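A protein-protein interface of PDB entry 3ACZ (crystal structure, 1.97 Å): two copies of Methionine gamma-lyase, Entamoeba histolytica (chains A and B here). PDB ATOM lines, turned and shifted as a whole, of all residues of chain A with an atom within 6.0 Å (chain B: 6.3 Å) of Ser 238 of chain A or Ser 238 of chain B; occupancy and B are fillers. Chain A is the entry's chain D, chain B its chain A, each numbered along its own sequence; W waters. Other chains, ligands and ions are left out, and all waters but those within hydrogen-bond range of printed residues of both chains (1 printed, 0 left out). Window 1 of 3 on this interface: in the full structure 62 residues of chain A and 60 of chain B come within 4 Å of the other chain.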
ATOM      1  N   ALA A  79      30.322  -7.451  -4.579  1.00  0.00           N
ATOM      2  CA  ALA A  79      29.788  -8.804  -4.537  1.00  0.00           C
ATOM      3  C   ALA A  79      28.276  -8.771  -4.751  1.00  0.00           C
ATOM      4  O   ALA A  79      27.613  -7.793  -4.399  1.00  0.00           O
ATOM      5  CB  ALA A  79      30.122  -9.492  -3.155  1.00  0.00           C
ATOM      6  N   PHE A  80      27.730  -9.861  -5.267  1.00  0.00           N
ATOM      7  CA  PHE A  80      26.311  -9.932  -5.653  1.00  0.00           C
ATOM      8  C   PHE A  80      25.709 -11.271  -5.260  1.00  0.00           C
ATOM      9  O   PHE A  80      26.438 -12.237  -5.010  1.00  0.00           O
ATOM     10  CB  PHE A  80      26.209  -9.787  -7.194  1.00  0.00           C
ATOM     11  CG  PHE A  80      26.638  -8.437  -7.693  1.00  0.00           C
ATOM     12  CD1 PHE A  80      25.738  -7.376  -7.711  1.00  0.00           C
ATOM     13  CD2 PHE A  80      27.950  -8.206  -8.088  1.00  0.00           C
ATOM     14  CE1 PHE A  80      26.130  -6.113  -8.168  1.00  0.00           C
ATOM     15  CE2 PHE A  80      28.348  -6.936  -8.561  1.00  0.00           C
ATOM     16  CZ  PHE A  80      27.440  -5.897  -8.580  1.00  0.00           C
ATOM     17  N   GLY A  81      24.390 -11.353  -5.299  1.00  0.00           N
ATOM     18  CA  GLY A  81      23.672 -12.595  -4.966  1.00  0.00           C
ATOM     19  C   GLY A  81      23.863 -13.702  -6.011  1.00  0.00           C
ATOM     20  O   GLY A  81      23.494 -14.841  -5.776  1.00  0.00           O
ATOM     21  N   SER A  82      24.422 -13.360  -7.167  1.00  0.00           N
ATOM     22  CA  SER A  82      24.672 -14.353  -8.231  1.00  0.00           C
ATOM     23  C   SER A  82      25.541 -13.750  -9.292  1.00  0.00           C
ATOM     24  O   SER A  82      25.655 -12.512  -9.375  1.00  0.00           O
ATOM     25  CB  SER A  82      23.338 -14.793  -8.882  1.00  0.00           C
ATOM     26  OG  SER A  82      22.704 -13.688  -9.507  1.00  0.00           O
ATOM     27  N   MET A  84      24.624 -13.628 -12.349  1.00  0.00           N
ATOM     28  CA  MET A  84      23.707 -12.790 -13.159  1.00  0.00           C
ATOM     29  C   MET A  84      23.547 -11.383 -12.590  1.00  0.00           C
ATOM     30  O   MET A  84      23.423 -10.410 -13.344  1.00  0.00           O
ATOM     31  CB  MET A  84      22.358 -13.475 -13.402  1.00  0.00           C
ATOM     32  CG  MET A  84      22.486 -14.729 -14.344  1.00  0.00           C
ATOM     33  SD  MET A  84      23.529 -14.539 -15.820  1.00  0.00           S
ATOM     34  CE  MET A  84      22.738 -13.092 -16.589  1.00  0.00           C
ATOM     35  N   GLY A  85      23.587 -11.277 -11.263  1.00  0.00           N
ATOM     36  CA  GLY A  85      23.548  -9.975 -10.594  1.00  0.00           C
ATOM     37  C   GLY A  85      24.768  -9.157 -10.968  1.00  0.00           C
ATOM     38  O   GLY A  85      24.649  -7.960 -11.296  1.00  0.00           O
ATOM     39  N   ALA A  86      25.951  -9.791 -10.980  1.00  0.00           N
ATOM     40  CA  ALA A  86      27.145  -9.079 -11.355  1.00  0.00           C
ATOM     41  C   ALA A  86      27.059  -8.655 -12.824  1.00  0.00           C
ATOM     42  O   ALA A  86      27.558  -7.572 -13.214  1.00  0.00           O
ATOM     43  CB  ALA A  86      28.403  -9.992 -11.142  1.00  0.00           C
ATOM     44  N   SER A  89      24.410  -5.933 -13.371  1.00  0.00           N
ATOM     45  CA  SER A  89      24.973  -4.717 -12.762  1.00  0.00           C
ATOM     46  C   SER A  89      26.182  -4.099 -13.469  1.00  0.00           C
ATOM     47  O   SER A  89      26.426  -2.902 -13.293  1.00  0.00           O
ATOM     48  CB  SER A  89      25.343  -4.941 -11.294  1.00  0.00           C
ATOM     49  OG  SER A  89      24.179  -5.264 -10.541  1.00  0.00           O
ATOM     50  N   ARG A 233      23.724  -1.415  -7.795  1.00  0.00           N
ATOM     51  CA  ARG A 233      23.439  -2.488  -6.828  1.00  0.00           C
ATOM     52  C   ARG A 233      22.522  -2.039  -5.687  1.00  0.00           C
ATOM     53  O   ARG A 233      21.591  -2.782  -5.284  1.00  0.00           O
ATOM     54  CB  ARG A 233      24.762  -3.092  -6.288  1.00  0.00           C
ATOM     55  CG  ARG A 233      24.523  -4.380  -5.419  1.00  0.00           C
ATOM     56  CD  ARG A 233      25.822  -4.885  -4.778  1.00  0.00           C
ATOM     57  NE  ARG A 233      26.347  -3.909  -3.829  1.00  0.00           N
ATOM     58  CZ  ARG A 233      27.508  -4.024  -3.181  1.00  0.00           C
ATOM     59  NH1 ARG A 233      27.863  -3.061  -2.330  1.00  0.00           N
ATOM     60  NH2 ARG A 233      28.302  -5.104  -3.371  1.00  0.00           N
ATOM     61  N   ALA A 236      19.131  -1.980  -7.578  1.00  0.00           N
ATOM     62  CA  ALA A 236      18.757  -3.263  -8.226  1.00  0.00           C
ATOM     63  C   ALA A 236      18.655  -4.403  -7.196  1.00  0.00           C
ATOM     64  O   ALA A 236      17.796  -5.303  -7.304  1.00  0.00           O
ATOM     65  CB  ALA A 236      19.747  -3.616  -9.329  1.00  0.00           C
ATOM     66  N   GLY A 237      19.535  -4.360  -6.202  1.00  0.00           N
ATOM     67  CA  GLY A 237      19.362  -5.183  -4.978  1.00  0.00           C
ATOM     68  C   GLY A 237      19.855  -6.632  -4.998  1.00  0.00           C
ATOM     69  O   GLY A 237      19.373  -7.456  -4.203  1.00  0.00           O
ATOM     70  N   SER A 238      20.769  -6.966  -5.916  1.00  0.00           N
ATOM     71  CA  SER A 238      21.375  -8.303  -5.905  1.00  0.00           C
ATOM     72  C   SER A 238      22.583  -8.300  -4.955  1.00  0.00           C
ATOM     73  O   SER A 238      23.665  -7.844  -5.302  1.00  0.00           O
ATOM     74  CB  SER A 238      21.787  -8.748  -7.301  1.00  0.00           C
ATOM     75  OG  SER A 238      22.439 -10.011  -7.225  1.00  0.00           O
ATOM     76  N   LEU A 239      22.377  -8.792  -3.740  1.00  0.00           N
ATOM     77  CA  LEU A 239      23.399  -8.748  -2.692  1.00  0.00           C
ATOM     78  C   LEU A 239      23.920 -10.138  -2.364  1.00  0.00           C
ATOM     79  O   LEU A 239      23.168 -11.124  -2.444  1.00  0.00           O
ATOM     80  CB  LEU A 239      22.795  -8.162  -1.407  1.00  0.00           C
ATOM     81  CG  LEU A 239      22.077  -6.815  -1.548  1.00  0.00           C
ATOM     82  CD1 LEU A 239      21.408  -6.421  -0.210  1.00  0.00           C
ATOM     83  CD2 LEU A 239      23.134  -5.752  -2.028  1.00  0.00           C
ATOM     84  N   MET A 240      25.172 -10.206  -1.921  1.00  0.00           N
ATOM     85  CA  MET A 240      25.690 -11.420  -1.328  1.00  0.00           C
ATOM     86  C   MET A 240      25.320 -11.435   0.166  1.00  0.00           C
ATOM     87  O   MET A 240      25.547 -10.456   0.890  1.00  0.00           O
ATOM     88  CB  MET A 240      27.214 -11.515  -1.567  1.00  0.00           C
ATOM     89  CG  MET A 240      27.853 -12.712  -0.897  1.00  0.00           C
ATOM     90  SD  MET A 240      29.581 -12.804  -1.355  1.00  0.00           S
ATOM     91  CE  MET A 240      29.494 -13.495  -3.019  1.00  0.00           C
ATOM     92  N   ALA B  79      10.983 -14.689  -3.734  1.00  0.00           N
ATOM     93  CA  ALA B  79      11.905 -14.070  -2.750  1.00  0.00           C
ATOM     94  C   ALA B  79      13.141 -13.488  -3.433  1.00  0.00           C
ATOM     95  O   ALA B  79      13.590 -14.021  -4.475  1.00  0.00           O
ATOM     96  CB  ALA B  79      12.351 -15.107  -1.737  1.00  0.00           C
ATOM     97  N   PHE B  80      13.703 -12.434  -2.840  1.00  0.00           N
ATOM     98  CA  PHE B  80      14.846 -11.690  -3.405  1.00  0.00           C
ATOM     99  C   PHE B  80      15.890 -11.413  -2.315  1.00  0.00           C
ATOM    100  O   PHE B  80      15.615 -11.549  -1.096  1.00  0.00           O
ATOM    101  CB  PHE B  80      14.372 -10.355  -4.048  1.00  0.00           C
ATOM    102  CG  PHE B  80      13.357 -10.545  -5.142  1.00  0.00           C
ATOM    103  CD1 PHE B  80      13.757 -10.666  -6.474  1.00  0.00           C
ATOM    104  CD2 PHE B  80      12.004 -10.638  -4.837  1.00  0.00           C
ATOM    105  CE1 PHE B  80      12.817 -10.874  -7.485  1.00  0.00           C
ATOM    106  CE2 PHE B  80      11.037 -10.855  -5.863  1.00  0.00           C
ATOM    107  CZ  PHE B  80      11.434 -10.960  -7.162  1.00  0.00           C
ATOM    108  N   GLY B  81      17.070 -10.988  -2.761  1.00  0.00           N
ATOM    109  CA  GLY B  81      18.167 -10.628  -1.885  1.00  0.00           C
ATOM    110  C   GLY B  81      17.853  -9.351  -1.102  1.00  0.00           C
ATOM    111  O   GLY B  81      18.554  -9.023  -0.152  1.00  0.00           O
ATOM    112  N   SER B  82      16.793  -8.640  -1.467  1.00  0.00           N
ATOM    113  CA  SER B  82      16.472  -7.386  -0.761  1.00  0.00           C
ATOM    114  C   SER B  82      15.112  -6.892  -1.234  1.00  0.00           C
ATOM    115  O   SER B  82      14.632  -7.326  -2.276  1.00  0.00           O
ATOM    116  CB  SER B  82      17.548  -6.309  -0.985  1.00  0.00           C
ATOM    117  OG  SER B  82      17.650  -5.936  -2.361  1.00  0.00           O
ATOM    118  N   MET B  84      14.701  -3.992  -2.349  1.00  0.00           N
ATOM    119  CA  MET B  84      14.974  -3.328  -3.617  1.00  0.00           C
ATOM    120  C   MET B  84      15.013  -4.325  -4.772  1.00  0.00           C
ATOM    121  O   MET B  84      14.590  -3.961  -5.870  1.00  0.00           O
ATOM    122  CB  MET B  84      16.257  -2.459  -3.593  1.00  0.00           C
ATOM    123  CG  MET B  84      16.151  -1.199  -2.658  1.00  0.00           C
ATOM    124  SD  MET B  84      14.596  -0.247  -2.818  1.00  0.00           S
ATOM    125  CE  MET B  84      14.626   0.197  -4.565  1.00  0.00           C
ATOM    126  N   GLY B  85      15.501  -5.563  -4.539  1.00  0.00           N
ATOM    127  CA  GLY B  85      15.442  -6.622  -5.562  1.00  0.00           C
ATOM    128  C   GLY B  85      13.984  -6.890  -5.944  1.00  0.00           C
ATOM    129  O   GLY B  85      13.648  -7.013  -7.139  1.00  0.00           O
ATOM    130  N   ALA B  86      13.120  -6.967  -4.935  1.00  0.00           N
ATOM    131  CA  ALA B  86      11.669  -7.163  -5.159  1.00  0.00           C
ATOM    132  C   ALA B  86      11.054  -6.004  -5.965  1.00  0.00           C
ATOM    133  O   ALA B  86      10.259  -6.243  -6.890  1.00  0.00           O
ATOM    134  CB  ALA B  86      10.922  -7.312  -3.818  1.00  0.00           C
ATOM    135  N   SER B  89      12.386  -5.913  -9.574  1.00  0.00           N
ATOM    136  CA  SER B  89      11.861  -7.066 -10.328  1.00  0.00           C
ATOM    137  C   SER B  89      10.342  -7.044 -10.540  1.00  0.00           C
ATOM    138  O   SER B  89       9.852  -7.773 -11.390  1.00  0.00           O
ATOM    139  CB  SER B  89      12.263  -8.399  -9.652  1.00  0.00           C
ATOM    140  OG  SER B  89      13.689  -8.534  -9.513  1.00  0.00           O
ATOM    141  N   ARG B 233      13.982 -12.218 -12.469  1.00  0.00           N
ATOM    142  CA  ARG B 233      14.887 -12.573 -11.371  1.00  0.00           C
ATOM    143  C   ARG B 233      16.023 -13.482 -11.828  1.00  0.00           C
ATOM    144  O   ARG B 233      17.197 -13.337 -11.396  1.00  0.00           O
ATOM    145  CB  ARG B 233      14.098 -13.256 -10.233  1.00  0.00           C
ATOM    146  CG  ARG B 233      14.980 -13.526  -9.005  1.00  0.00           C
ATOM    147  CD  ARG B 233      14.242 -14.246  -7.886  1.00  0.00           C
ATOM    148  NE  ARG B 233      13.873 -15.597  -8.315  1.00  0.00           N
ATOM    149  CZ  ARG B 233      13.121 -16.432  -7.601  1.00  0.00           C
ATOM    150  NH1 ARG B 233      12.812 -17.630  -8.091  1.00  0.00           N
ATOM    151  NH2 ARG B 233      12.657 -16.077  -6.406  1.00  0.00           N
ATOM    152  N   ALA B 236      18.285 -10.980 -13.748  1.00  0.00           N
ATOM    153  CA  ALA B 236      18.750  -9.842 -12.947  1.00  0.00           C
ATOM    154  C   ALA B 236      19.481 -10.315 -11.680  1.00  0.00           C
ATOM    155  O   ALA B 236      20.359  -9.638 -11.173  1.00  0.00           O
ATOM    156  CB  ALA B 236      17.595  -8.924 -12.583  1.00  0.00           C
ATOM    157  N   GLY B 237      19.101 -11.470 -11.154  1.00  0.00           N
ATOM    158  CA  GLY B 237      19.971 -12.131 -10.177  1.00  0.00           C
ATOM    159  C   GLY B 237      19.901 -11.721  -8.706  1.00  0.00           C
ATOM    160  O   GLY B 237      20.814 -12.064  -7.944  1.00  0.00           O
ATOM    161  N   SER B 238      18.856 -10.993  -8.301  1.00  0.00           N
ATOM    162  CA  SER B 238      18.630 -10.753  -6.857  1.00  0.00           C
ATOM    163  C   SER B 238      17.981 -11.940  -6.163  1.00  0.00           C
ATOM    164  O   SER B 238      16.772 -12.105  -6.216  1.00  0.00           O
ATOM    165  CB  SER B 238      17.838  -9.469  -6.569  1.00  0.00           C
ATOM    166  OG  SER B 238      17.686  -9.296  -5.141  1.00  0.00           O
ATOM    167  N   LEU B 239      18.800 -12.762  -5.495  1.00  0.00           N
ATOM    168  CA  LEU B 239      18.320 -14.013  -4.877  1.00  0.00           C
ATOM    169  C   LEU B 239      18.351 -13.951  -3.365  1.00  0.00           C
ATOM    170  O   LEU B 239      19.255 -13.339  -2.754  1.00  0.00           O
ATOM    171  CB  LEU B 239      19.224 -15.191  -5.308  1.00  0.00           C
ATOM    172  CG  LEU B 239      19.472 -15.311  -6.800  1.00  0.00           C
ATOM    173  CD1 LEU B 239      20.454 -16.477  -7.019  1.00  0.00           C
ATOM    174  CD2 LEU B 239      18.097 -15.507  -7.526  1.00  0.00           C
ATOM    175  N   MET B 240      17.417 -14.648  -2.739  1.00  0.00           N
ATOM    176  CA  MET B 240      17.508 -14.832  -1.296  1.00  0.00           C
ATOM    177  C   MET B 240      18.389 -16.054  -1.083  1.00  0.00           C
ATOM    178  O   MET B 240      18.105 -17.109  -1.664  1.00  0.00           O
ATOM    179  CB  MET B 240      16.124 -15.066  -0.687  1.00  0.00           C
ATOM    180  CG  MET B 240      16.158 -15.336   0.809  1.00  0.00           C
ATOM    181  SD  MET B 240      14.466 -15.394   1.458  1.00  0.00           S
ATOM    182  CE  MET B 240      14.069 -13.643   1.584  1.00  0.00           C
HETATM  183  O   HOH W   1      20.795 -11.270  -3.824  1.00  0.00           O
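Water W1 bridges O of Leu 239 of chain A (2.7 Å) and O of Leu 239 of chain B (2.8 Å).
Of the 14 printed residues of chain B, 8 touch a printed residue of chain A. Printed residues of chain B that touch a printed residue of chain A: Gly 81, Ser 82, Met 84, Gly 85, Ala 236, Gly 237, Ser 238 and Leu 239. Hydrophobic or aromatic side chains of chain B within 4 Å of the printed part of chain A: Leu 239. Of the 14 printed residues of chain A, 8 touch a printed residue of chain B. Printed residues of chain A that touch a printed residue of chain B: Gly 81, Ser 82, Met 84, Gly 85, Ala 236, Gly 237, Ser 238 and Leu 239. Hydrophobic or aromatic side chains of chain A within 4 Å of the printed part of chain B: Leu 239.
N of Gly 81 of chain A sits close to O of Leu 239 of chain A (3.1 Å). The backbone NH (N) of Gly 81 of chain A lies within hydrogen-bond range of the side-chain hydroxyl (OG) of Ser 238 of chain A (3.1 Å). The backbone NH of Met 84 of chain A sits close to the side-chain hydroxyl of Ser 82 of chain A (3.4 Å). The backbone carbonyl oxygen (O) of Leu 239 of chain B lies close to the backbone NH (N) of Gly 81 of chain B (3.2 Å). The backbone NH (N) of Gly 85 of chain A sits at hydrogen-bond distance from the side-chain hydroxyl (OG) of Ser 82 of chain A. OG of Ser 238 of chain B is in hydrogen-bond range of N of Gly 81 of chain B, 3.0 Å away.
Among the printed residues, pairs that only touch across the chains: Gly 81 of chain A with Gly 237 of chain B, Gly 81 of chain A with Leu 239 of chain B, Ser 82 of chain A with Leu 239 of chain B, Met 84 of chain A with Ala 236 of chain B, Gly 85 of chain A with Ala 236 of chain B, Gly 85 of chain A with Gly 237 of chain B, Ala 236 of chain A with Met 84 of chain B, Ala 236 of chain A with Gly 85 of chain B, Gly 237 of chain A with Gly 81 of chain B, Gly 237 of chain A with Gly 85 of chain B, Ser 238 of chain A with Ser 238 of chain B, Leu 239 of chain A with Gly 81 of chain B and Leu 239 of chain A with Ser 82 of chain B.
OG of Ser 82 of chain A lies within hydrogen-bond range of O of Gly 237 of chain B, at 2.9 Å. The side-chain hydroxyl (OG) of Ser 82 of chain B sits at hydrogen-bond distance from the backbone carbonyl oxygen (O) of Gly 237 of chain A. The side-chain hydroxyl (OG) of Ser 238 of chain B sits at hydrogen-bond distance from the backbone carbonyl oxygen (O) of Gly 237 of chain A. The backbone carbonyl oxygen (O) of Gly 237 of chain B is in hydrogen-bond range of the side-chain hydroxyl (OG) of Ser 238 of chain A, at 2.7 Å.
Of chain B, only Gly 237 (2.7 Å) and Ser 238 (3.8 Å) come within 4 Å of Ser 238 of chain A. Of chain A, only Gly 237 and Ser 238 come within 4 Å of Ser 238 of chain B. Of the printed residues of chain A, Met 84 of chain B touches Ala 236. Printed residues of chain A within 4 Å of Ala 236 of chain B: Met 84 (3.8 Å) and Gly 85 (3.3 Å). Of the printed residues of chain A, Leu 239 of chain B touches Gly 81 (3.7 Å) and Ser 82 (3.8 Å). The nearest residue of chain B that does not touch Ser 238 of chain A is Ala 236 of chain B (4.2 Å).
Gly 81 of chain A touches Gly 237 of chain B, and with the chains exchanged Gly 237 of chain A touches Gly 81 of chain B. Met 84 of chain A touches Ala 236 of chain B, and with the chains exchanged Ala 236 of chain A touches Met 84 of chain B. Gly 85 of chain A touches Gly 237 of chain B, and with the chains exchanged Gly 237 of chain A touches Gly 85 of chain B. Ser 238 of chain B touches its own counterpart, Ser 238 of chain A. Of the 17 pairs that touch across the chains among the printed residues, 17 have their exchanged pair printed and touching as well.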
